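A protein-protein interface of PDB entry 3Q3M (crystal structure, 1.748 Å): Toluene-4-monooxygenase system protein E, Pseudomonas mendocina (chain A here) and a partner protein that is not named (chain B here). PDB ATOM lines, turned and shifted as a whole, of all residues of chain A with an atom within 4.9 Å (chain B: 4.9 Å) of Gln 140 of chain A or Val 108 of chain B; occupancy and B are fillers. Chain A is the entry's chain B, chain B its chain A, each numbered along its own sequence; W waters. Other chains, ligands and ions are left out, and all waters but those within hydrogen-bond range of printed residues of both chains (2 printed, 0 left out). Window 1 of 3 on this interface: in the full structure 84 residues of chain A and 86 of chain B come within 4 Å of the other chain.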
ATOM      1  N   HIS A  33      18.755  -5.623  24.720  1.00  0.00           N
ATOM      2  CA  HIS A  33      19.922  -5.318  23.851  1.00  0.00           C
ATOM      3  C   HIS A  33      20.276  -3.835  23.938  1.00  0.00           C
ATOM      4  O   HIS A  33      19.709  -3.028  23.204  1.00  0.00           O
ATOM      5  CB  HIS A  33      19.635  -5.600  22.375  1.00  0.00           C
ATOM      6  CG  HIS A  33      19.578  -7.055  22.016  1.00  0.00           C
ATOM      7  ND1 HIS A  33      20.235  -8.033  22.734  1.00  0.00           N
ATOM      8  CD2 HIS A  33      18.981  -7.689  20.980  1.00  0.00           C
ATOM      9  CE1 HIS A  33      20.027  -9.211  22.171  1.00  0.00           C
ATOM     10  NE2 HIS A  33      19.275  -9.029  21.100  1.00  0.00           N
ATOM     11  N   SER A 136      20.906 -20.842  13.908  1.00  0.00           N
ATOM     12  CA  SER A 136      20.021 -20.239  14.906  1.00  0.00           C
ATOM     13  C   SER A 136      20.821 -19.366  15.870  1.00  0.00           C
ATOM     14  O   SER A 136      20.352 -18.310  16.288  1.00  0.00           O
ATOM     15  CB  SER A 136      19.256 -21.304  15.690  1.00  0.00           C
ATOM     16  OG  SER A 136      18.407 -22.061  14.834  1.00  0.00           O
ATOM     17  N   ALA A 137      22.028 -19.809  16.206  1.00  0.00           N
ATOM     18  CA  ALA A 137      22.892 -19.045  17.090  1.00  0.00           C
ATOM     19  C   ALA A 137      23.297 -17.736  16.405  1.00  0.00           C
ATOM     20  O   ALA A 137      23.462 -16.687  17.073  1.00  0.00           O
ATOM     21  CB  ALA A 137      24.140 -19.885  17.501  1.00  0.00           C
ATOM     22  N   TYR A 138      23.443 -17.771  15.082  1.00  0.00           N
ATOM     23  CA  TYR A 138      23.784 -16.539  14.359  1.00  0.00           C
ATOM     24  C   TYR A 138      22.630 -15.526  14.430  1.00  0.00           C
ATOM     25  O   TYR A 138      22.841 -14.340  14.702  1.00  0.00           O
ATOM     26  CB  TYR A 138      24.201 -16.777  12.887  1.00  0.00           C
ATOM     27  CG  TYR A 138      24.671 -15.468  12.272  1.00  0.00           C
ATOM     28  CD1 TYR A 138      23.900 -14.787  11.334  1.00  0.00           C
ATOM     29  CD2 TYR A 138      25.856 -14.877  12.707  1.00  0.00           C
ATOM     30  CE1 TYR A 138      24.333 -13.545  10.816  1.00  0.00           C
ATOM     31  CE2 TYR A 138      26.286 -13.650  12.201  1.00  0.00           C
ATOM     32  CZ  TYR A 138      25.537 -12.997  11.255  1.00  0.00           C
ATOM     33  OH  TYR A 138      25.979 -11.777  10.784  1.00  0.00           O
ATOM     34  N   VAL A 139      21.411 -15.982  14.194  1.00  0.00           N
ATOM     35  CA  VAL A 139      20.274 -15.059  14.273  1.00  0.00           C
ATOM     36  C   VAL A 139      20.173 -14.500  15.694  1.00  0.00           C
ATOM     37  O   VAL A 139      19.911 -13.310  15.875  1.00  0.00           O
ATOM     38  CB  VAL A 139      18.940 -15.714  13.825  1.00  0.00           C
ATOM     39  CG1 VAL A 139      17.832 -14.644  13.751  1.00  0.00           C
ATOM     40  CG2 VAL A 139      19.109 -16.358  12.446  1.00  0.00           C
ATOM     41  N   GLN A 140      20.389 -15.349  16.700  1.00  0.00           N
ATOM     42  CA  GLN A 140      20.417 -14.883  18.094  1.00  0.00           C
ATOM     43  C   GLN A 140      21.318 -13.669  18.283  1.00  0.00           C
ATOM     44  O   GLN A 140      20.891 -12.648  18.839  1.00  0.00           O
ATOM     45  CB  GLN A 140      20.887 -16.024  19.051  1.00  0.00           C
ATOM     46  CG  GLN A 140      21.145 -15.583  20.517  1.00  0.00           C
ATOM     47  CD  GLN A 140      22.520 -14.957  20.699  1.00  0.00           C
ATOM     48  OE1 GLN A 140      23.532 -15.501  20.229  1.00  0.00           O
ATOM     49  NE2 GLN A 140      22.568 -13.812  21.374  1.00  0.00           N
ATOM     50  N   GLN A 141      22.570 -13.785  17.836  1.00  0.00           N
ATOM     51  CA  GLN A 141      23.563 -12.764  18.168  1.00  0.00           C
ATOM     52  C   GLN A 141      23.375 -11.480  17.364  1.00  0.00           C
ATOM     53  O   GLN A 141      23.835 -10.428  17.780  1.00  0.00           O
ATOM     54  CB  GLN A 141      25.003 -13.321  18.074  1.00  0.00           C
ATOM     55  CG  GLN A 141      25.433 -13.664  16.647  1.00  0.00           C
ATOM     56  CD  GLN A 141      26.568 -14.669  16.626  1.00  0.00           C
ATOM     57  OE1 GLN A 141      27.715 -14.331  16.308  1.00  0.00           O
ATOM     58  NE2 GLN A 141      26.248 -15.917  16.953  1.00  0.00           N
ATOM     59  N   MET A 142      22.622 -11.552  16.263  1.00  0.00           N
ATOM     60  CA  MET A 142      22.436 -10.401  15.384  1.00  0.00           C
ATOM     61  C   MET A 142      21.068  -9.699  15.516  1.00  0.00           C
ATOM     62  O   MET A 142      20.944  -8.535  15.132  1.00  0.00           O
ATOM     63  CB  MET A 142      22.630 -10.811  13.902  1.00  0.00           C
ATOM     64  CG  MET A 142      24.054 -11.259  13.541  1.00  0.00           C
ATOM     65  SD  MET A 142      25.413 -10.246  14.178  1.00  0.00           S
ATOM     66  CE  MET A 142      25.011  -8.637  13.511  1.00  0.00           C
ATOM     67  N   ALA A 143      20.051 -10.395  16.038  1.00  0.00           N
ATOM     68  CA  ALA A 143      18.685  -9.852  16.034  1.00  0.00           C
ATOM     69  C   ALA A 143      18.582  -8.548  16.809  1.00  0.00           C
ATOM     70  O   ALA A 143      19.250  -8.379  17.827  1.00  0.00           O
ATOM     71  CB  ALA A 143      17.703 -10.881  16.608  1.00  0.00           C
ATOM     72  N   SER A 149      15.837 -12.475  19.968  1.00  0.00           N
ATOM     73  CA  SER A 149      17.018 -13.277  20.279  1.00  0.00           C
ATOM     74  C   SER A 149      16.656 -14.460  21.188  1.00  0.00           C
ATOM     75  O   SER A 149      17.188 -15.558  21.028  1.00  0.00           O
ATOM     76  CB  SER A 149      18.147 -12.416  20.880  1.00  0.00           C
ATOM     77  OG  SER A 149      18.678 -11.512  19.901  1.00  0.00           O
ATOM     78  N   CYS A 152      15.389 -17.363  19.305  1.00  0.00           N
ATOM     79  CA  CYS A 152      16.518 -18.000  18.641  1.00  0.00           C
ATOM     80  C   CYS A 152      17.393 -18.841  19.573  1.00  0.00           C
ATOM     81  O   CYS A 152      17.942 -19.858  19.144  1.00  0.00           O
ATOM     82  CB  CYS A 152      17.403 -16.944  17.958  1.00  0.00           C
ATOM     83  SG  CYS A 152      16.570 -16.018  16.666  1.00  0.00           S
ATOM     84  N   ILE A 153      17.546 -18.419  20.827  1.00  0.00           N
ATOM     85  CA  ILE A 153      18.337 -19.215  21.789  1.00  0.00           C
ATOM     86  C   ILE A 153      17.645 -20.554  21.970  1.00  0.00           C
ATOM     87  O   ILE A 153      18.263 -21.627  21.899  1.00  0.00           O
ATOM     88  CB  ILE A 153      18.465 -18.529  23.172  1.00  0.00           C
ATOM     89  CG1 ILE A 153      19.222 -17.187  23.049  1.00  0.00           C
ATOM     90  CG2 ILE A 153      19.202 -19.444  24.195  1.00  0.00           C
ATOM     91  CD1 ILE A 153      19.003 -16.276  24.271  1.00  0.00           C
ATOM     92  N   GLU B 104      25.065 -10.294  32.123  1.00  0.00           N
ATOM     93  CA  GLU B 104      24.823 -11.731  31.932  1.00  0.00           C
ATOM     94  C   GLU B 104      24.088 -11.969  30.619  1.00  0.00           C
ATOM     95  O   GLU B 104      24.448 -12.853  29.823  1.00  0.00           O
ATOM     96  CB  GLU B 104      23.940 -12.269  33.064  1.00  0.00           C
ATOM     97  CG  GLU B 104      24.591 -12.187  34.423  1.00  0.00           C
ATOM     98  CD  GLU B 104      25.273 -13.468  34.809  1.00  0.00           C
ATOM     99  OE1 GLU B 104      25.453 -13.669  36.022  1.00  0.00           O
ATOM    100  OE2 GLU B 104      25.636 -14.255  33.897  1.00  0.00           O
ATOM    101  N   TYR B 105      23.047 -11.182  30.368  1.00  0.00           N
ATOM    102  CA  TYR B 105      22.328 -11.371  29.107  1.00  0.00           C
ATOM    103  C   TYR B 105      23.243 -11.117  27.879  1.00  0.00           C
ATOM    104  O   TYR B 105      23.162 -11.814  26.856  1.00  0.00           O
ATOM    105  CB  TYR B 105      21.063 -10.508  29.060  1.00  0.00           C
ATOM    106  CG  TYR B 105      20.248 -10.857  27.852  1.00  0.00           C
ATOM    107  CD1 TYR B 105      19.463 -12.011  27.829  1.00  0.00           C
ATOM    108  CD2 TYR B 105      20.295 -10.061  26.710  1.00  0.00           C
ATOM    109  CE1 TYR B 105      18.753 -12.355  26.684  1.00  0.00           C
ATOM    110  CE2 TYR B 105      19.577 -10.386  25.576  1.00  0.00           C
ATOM    111  CZ  TYR B 105      18.808 -11.525  25.571  1.00  0.00           C
ATOM    112  OH  TYR B 105      18.105 -11.891  24.430  1.00  0.00           O
ATOM    113  N   ALA B 106      24.142 -10.145  27.988  1.00  0.00           N
ATOM    114  CA  ALA B 106      25.113  -9.923  26.909  1.00  0.00           C
ATOM    115  C   ALA B 106      26.028 -11.134  26.713  1.00  0.00           C
ATOM    116  O   ALA B 106      26.435 -11.420  25.584  1.00  0.00           O
ATOM    117  CB  ALA B 106      25.944  -8.665  27.174  1.00  0.00           C
ATOM    118  N   ALA B 107      26.342 -11.841  27.796  1.00  0.00           N
ATOM    119  CA  ALA B 107      27.199 -13.011  27.686  1.00  0.00           C
ATOM    120  C   ALA B 107      26.563 -14.086  26.807  1.00  0.00           C
ATOM    121  O   ALA B 107      27.273 -14.944  26.285  1.00  0.00           O
ATOM    122  CB  ALA B 107      27.545 -13.596  29.059  1.00  0.00           C
ATOM    123  N   VAL B 108      25.231 -14.065  26.665  1.00  0.00           N
ATOM    124  CA  VAL B 108      24.596 -14.982  25.725  1.00  0.00           C
ATOM    125  C   VAL B 108      25.256 -14.840  24.351  1.00  0.00           C
ATOM    126  O   VAL B 108      25.490 -15.818  23.644  1.00  0.00           O
ATOM    127  CB  VAL B 108      23.093 -14.729  25.580  1.00  0.00           C
ATOM    128  CG1 VAL B 108      22.539 -15.649  24.489  1.00  0.00           C
ATOM    129  CG2 VAL B 108      22.405 -14.994  26.941  1.00  0.00           C
ATOM    130  N   THR B 109      25.548 -13.602  23.989  1.00  0.00           N
ATOM    131  CA  THR B 109      26.135 -13.292  22.687  1.00  0.00           C
ATOM    132  C   THR B 109      27.578 -13.772  22.570  1.00  0.00           C
ATOM    133  O   THR B 109      27.989 -14.249  21.504  1.00  0.00           O
ATOM    134  CB  THR B 109      26.004 -11.778  22.356  1.00  0.00           C
ATOM    135  OG1 THR B 109      24.622 -11.484  22.119  1.00  0.00           O
ATOM    136  CG2 THR B 109      26.822 -11.413  21.117  1.00  0.00           C
ATOM    137  N   GLY B 110      28.341 -13.677  23.656  1.00  0.00           N
ATOM    138  CA  GLY B 110      29.676 -14.280  23.668  1.00  0.00           C
ATOM    139  C   GLY B 110      29.583 -15.777  23.357  1.00  0.00           C
ATOM    140  O   GLY B 110      30.313 -16.311  22.508  1.00  0.00           O
ATOM    141  N   GLU B 111      28.685 -16.462  24.061  1.00  0.00           N
ATOM    142  CA  GLU B 111      28.455 -17.892  23.852  1.00  0.00           C
ATOM    143  C   GLU B 111      27.942 -18.165  22.435  1.00  0.00           C
ATOM    144  O   GLU B 111      28.406 -19.090  21.758  1.00  0.00           O
ATOM    145  CB  GLU B 111      27.503 -18.447  24.913  1.00  0.00           C
ATOM    146  CG  GLU B 111      28.067 -18.429  26.348  1.00  0.00           C
ATOM    147  CD  GLU B 111      29.160 -19.487  26.596  1.00  0.00           C
ATOM    148  OE1 GLU B 111      29.305 -20.414  25.787  1.00  0.00           O
ATOM    149  OE2 GLU B 111      29.862 -19.402  27.617  1.00  0.00           O
ATOM    150  N   GLY B 112      27.031 -17.323  21.959  1.00  0.00           N
ATOM    151  CA  GLY B 112      26.529 -17.449  20.596  1.00  0.00           C
ATOM    152  C   GLY B 112      27.628 -17.302  19.556  1.00  0.00           C
ATOM    153  O   GLY B 112      27.623 -17.973  18.506  1.00  0.00           O
ATOM    154  N   MET B 131      24.917 -20.559  26.043  1.00  0.00           N
ATOM    155  CA  MET B 131      23.917 -19.557  25.667  1.00  0.00           C
ATOM    156  C   MET B 131      22.728 -19.668  26.616  1.00  0.00           C
ATOM    157  O   MET B 131      22.176 -18.677  27.092  1.00  0.00           O
ATOM    158  CB  MET B 131      23.412 -19.811  24.237  1.00  0.00           C
ATOM    159  CG  MET B 131      24.448 -19.469  23.120  1.00  0.00           C
ATOM    160  SD  MET B 131      23.941 -20.087  21.513  1.00  0.00           S
ATOM    161  CE  MET B 131      22.573 -18.984  21.144  1.00  0.00           C
ATOM    162  N   GLU B 134      23.542 -18.458  30.229  1.00  0.00           N
ATOM    163  CA  GLU B 134      23.564 -16.997  30.393  1.00  0.00           C
ATOM    164  C   GLU B 134      22.157 -16.411  30.303  1.00  0.00           C
ATOM    165  O   GLU B 134      21.852 -15.427  30.969  1.00  0.00           O
ATOM    166  CB  GLU B 134      24.523 -16.305  29.404  1.00  0.00           C
ATOM    167  CG  GLU B 134      25.999 -16.768  29.509  1.00  0.00           C
ATOM    168  CD  GLU B 134      26.655 -16.680  30.902  1.00  0.00           C
ATOM    169  OE1 GLU B 134      26.043 -16.257  31.894  1.00  0.00           O
ATOM    170  OE2 GLU B 134      27.839 -17.055  30.995  1.00  0.00           O
ATOM    171  N   LEU B 135      21.303 -17.008  29.480  1.00  0.00           N
ATOM    172  CA  LEU B 135      19.883 -16.627  29.477  1.00  0.00           C
ATOM    173  C   LEU B 135      19.289 -16.796  30.872  1.00  0.00           C
ATOM    174  O   LEU B 135      18.594 -15.912  31.374  1.00  0.00           O
ATOM    175  CB  LEU B 135      19.103 -17.466  28.481  1.00  0.00           C
ATOM    176  CG  LEU B 135      17.600 -17.144  28.327  1.00  0.00           C
ATOM    177  CD1 LEU B 135      17.368 -15.767  27.827  1.00  0.00           C
ATOM    178  CD2 LEU B 135      16.956 -18.130  27.385  1.00  0.00           C
HETATM  179  O   HOH W   1      20.731 -12.473  23.075  1.00  0.00           O
HETATM  180  O   HOH W   2      24.219  -9.466  20.332  1.00  0.00           O
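The side-chain hydroxyl (OG1) of Thr 109 of chain B sits at hydrogen-bond distance from the side-chain amide nitrogen (NE2) of Gln 140 of chain A, at 3.2 Å. O of Gly 112 of chain B sits at hydrogen-bond distance from NE2 of Gln 141 of chain A, at 2.9 Å.
A ring nitrogen (NE2) of His 33 of chain A sits close to the backbone carbonyl oxygen (O) of Ala 143 of chain A, at 3.3 Å. NE2 of His 33 of chain A lies within hydrogen-bond range of OG of Ser 149 of chain A (2.8 Å). The backbone carbonyl oxygen of Ala 137 of chain A lies close to the side-chain amide oxygen of Gln 140 of chain A, 3.4 Å away. The backbone carbonyl oxygen (O) of Ala 137 of chain A is in hydrogen-bond range of the side-chain amide nitrogen (NE2) of Gln 141 of chain A, at 2.9 Å. O of Gln 140 of chain A sits at hydrogen-bond distance from OG of Ser 149 of chain A, at 2.7 Å.
Among the printed residues, merely in contact across the chains: Ser 149 of chain A with Tyr 105 of chain B (3.6 Å), Gln 140 of chain A with Gly 112 of chain B (3.6 Å), Ile 153 of chain A with Val 108 of chain B (3.6 Å), Gln 140 of chain A with Val 108 of chain B (3.6 Å), His 33 of chain A with Tyr 105 of chain B (3.6 Å), Gln 140 of chain A with Met 131 of chain B (3.7 Å) and Ile 153 of chain A with Leu 135 of chain B (3.9 Å).
Printed residues of chain B within 4 Å of Gln 140 of chain A: Val 108 (3.6 Å), Thr 109 (3.2 Å), Gly 112 (3.6 Å) and Met 131 (3.7 Å). Of the printed residues of chain B, Ile 153 of chain A touches Val 108 (3.6 Å) and Leu 135 (3.9 Å). Of chain A, only Gln 140 (3.6 Å) and Ile 153 (3.6 Å) come within 4 Å of Val 108 of chain B. Of the printed residues of chain A, Thr 109 of chain B touches Gln 140. Glu 111 of chain B touches none of the printed residues of chain A. Of the printed residues of chain A, Gly 112 of chain B touches Gln 140 and Gln 141. Of the printed residues of chain A, Leu 135 of chain B touches Ile 153. The nearest printed residue of chain B that does not touch Gln 140 of chain A is Glu 111 of chain B (5.6 Å). The nearest printed residue of chain A that does not touch Val 108 of chain B is Gln 141 of chain A (6.1 Å).
Hydrophobic or aromatic side chains of chain B within 4 Å of the printed part of chain A: Tyr 105, Val 108, Met 131 and Leu 135. Among the printed residues, no Asp or Glu carboxylate lies within 4 Å of a Lys or Arg side-chain nitrogen of the other chain.
Water W2 bridges OG1 of Thr 109 of chain B (2.7 Å) and O of Gln 141 of chain A (2.8 Å). Water W1 bridges the side-chain amide nitrogen of Gln 140 of chain A (2.8 Å) and the side-chain hydroxyl of Tyr 105 of chain B (3.0 Å).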
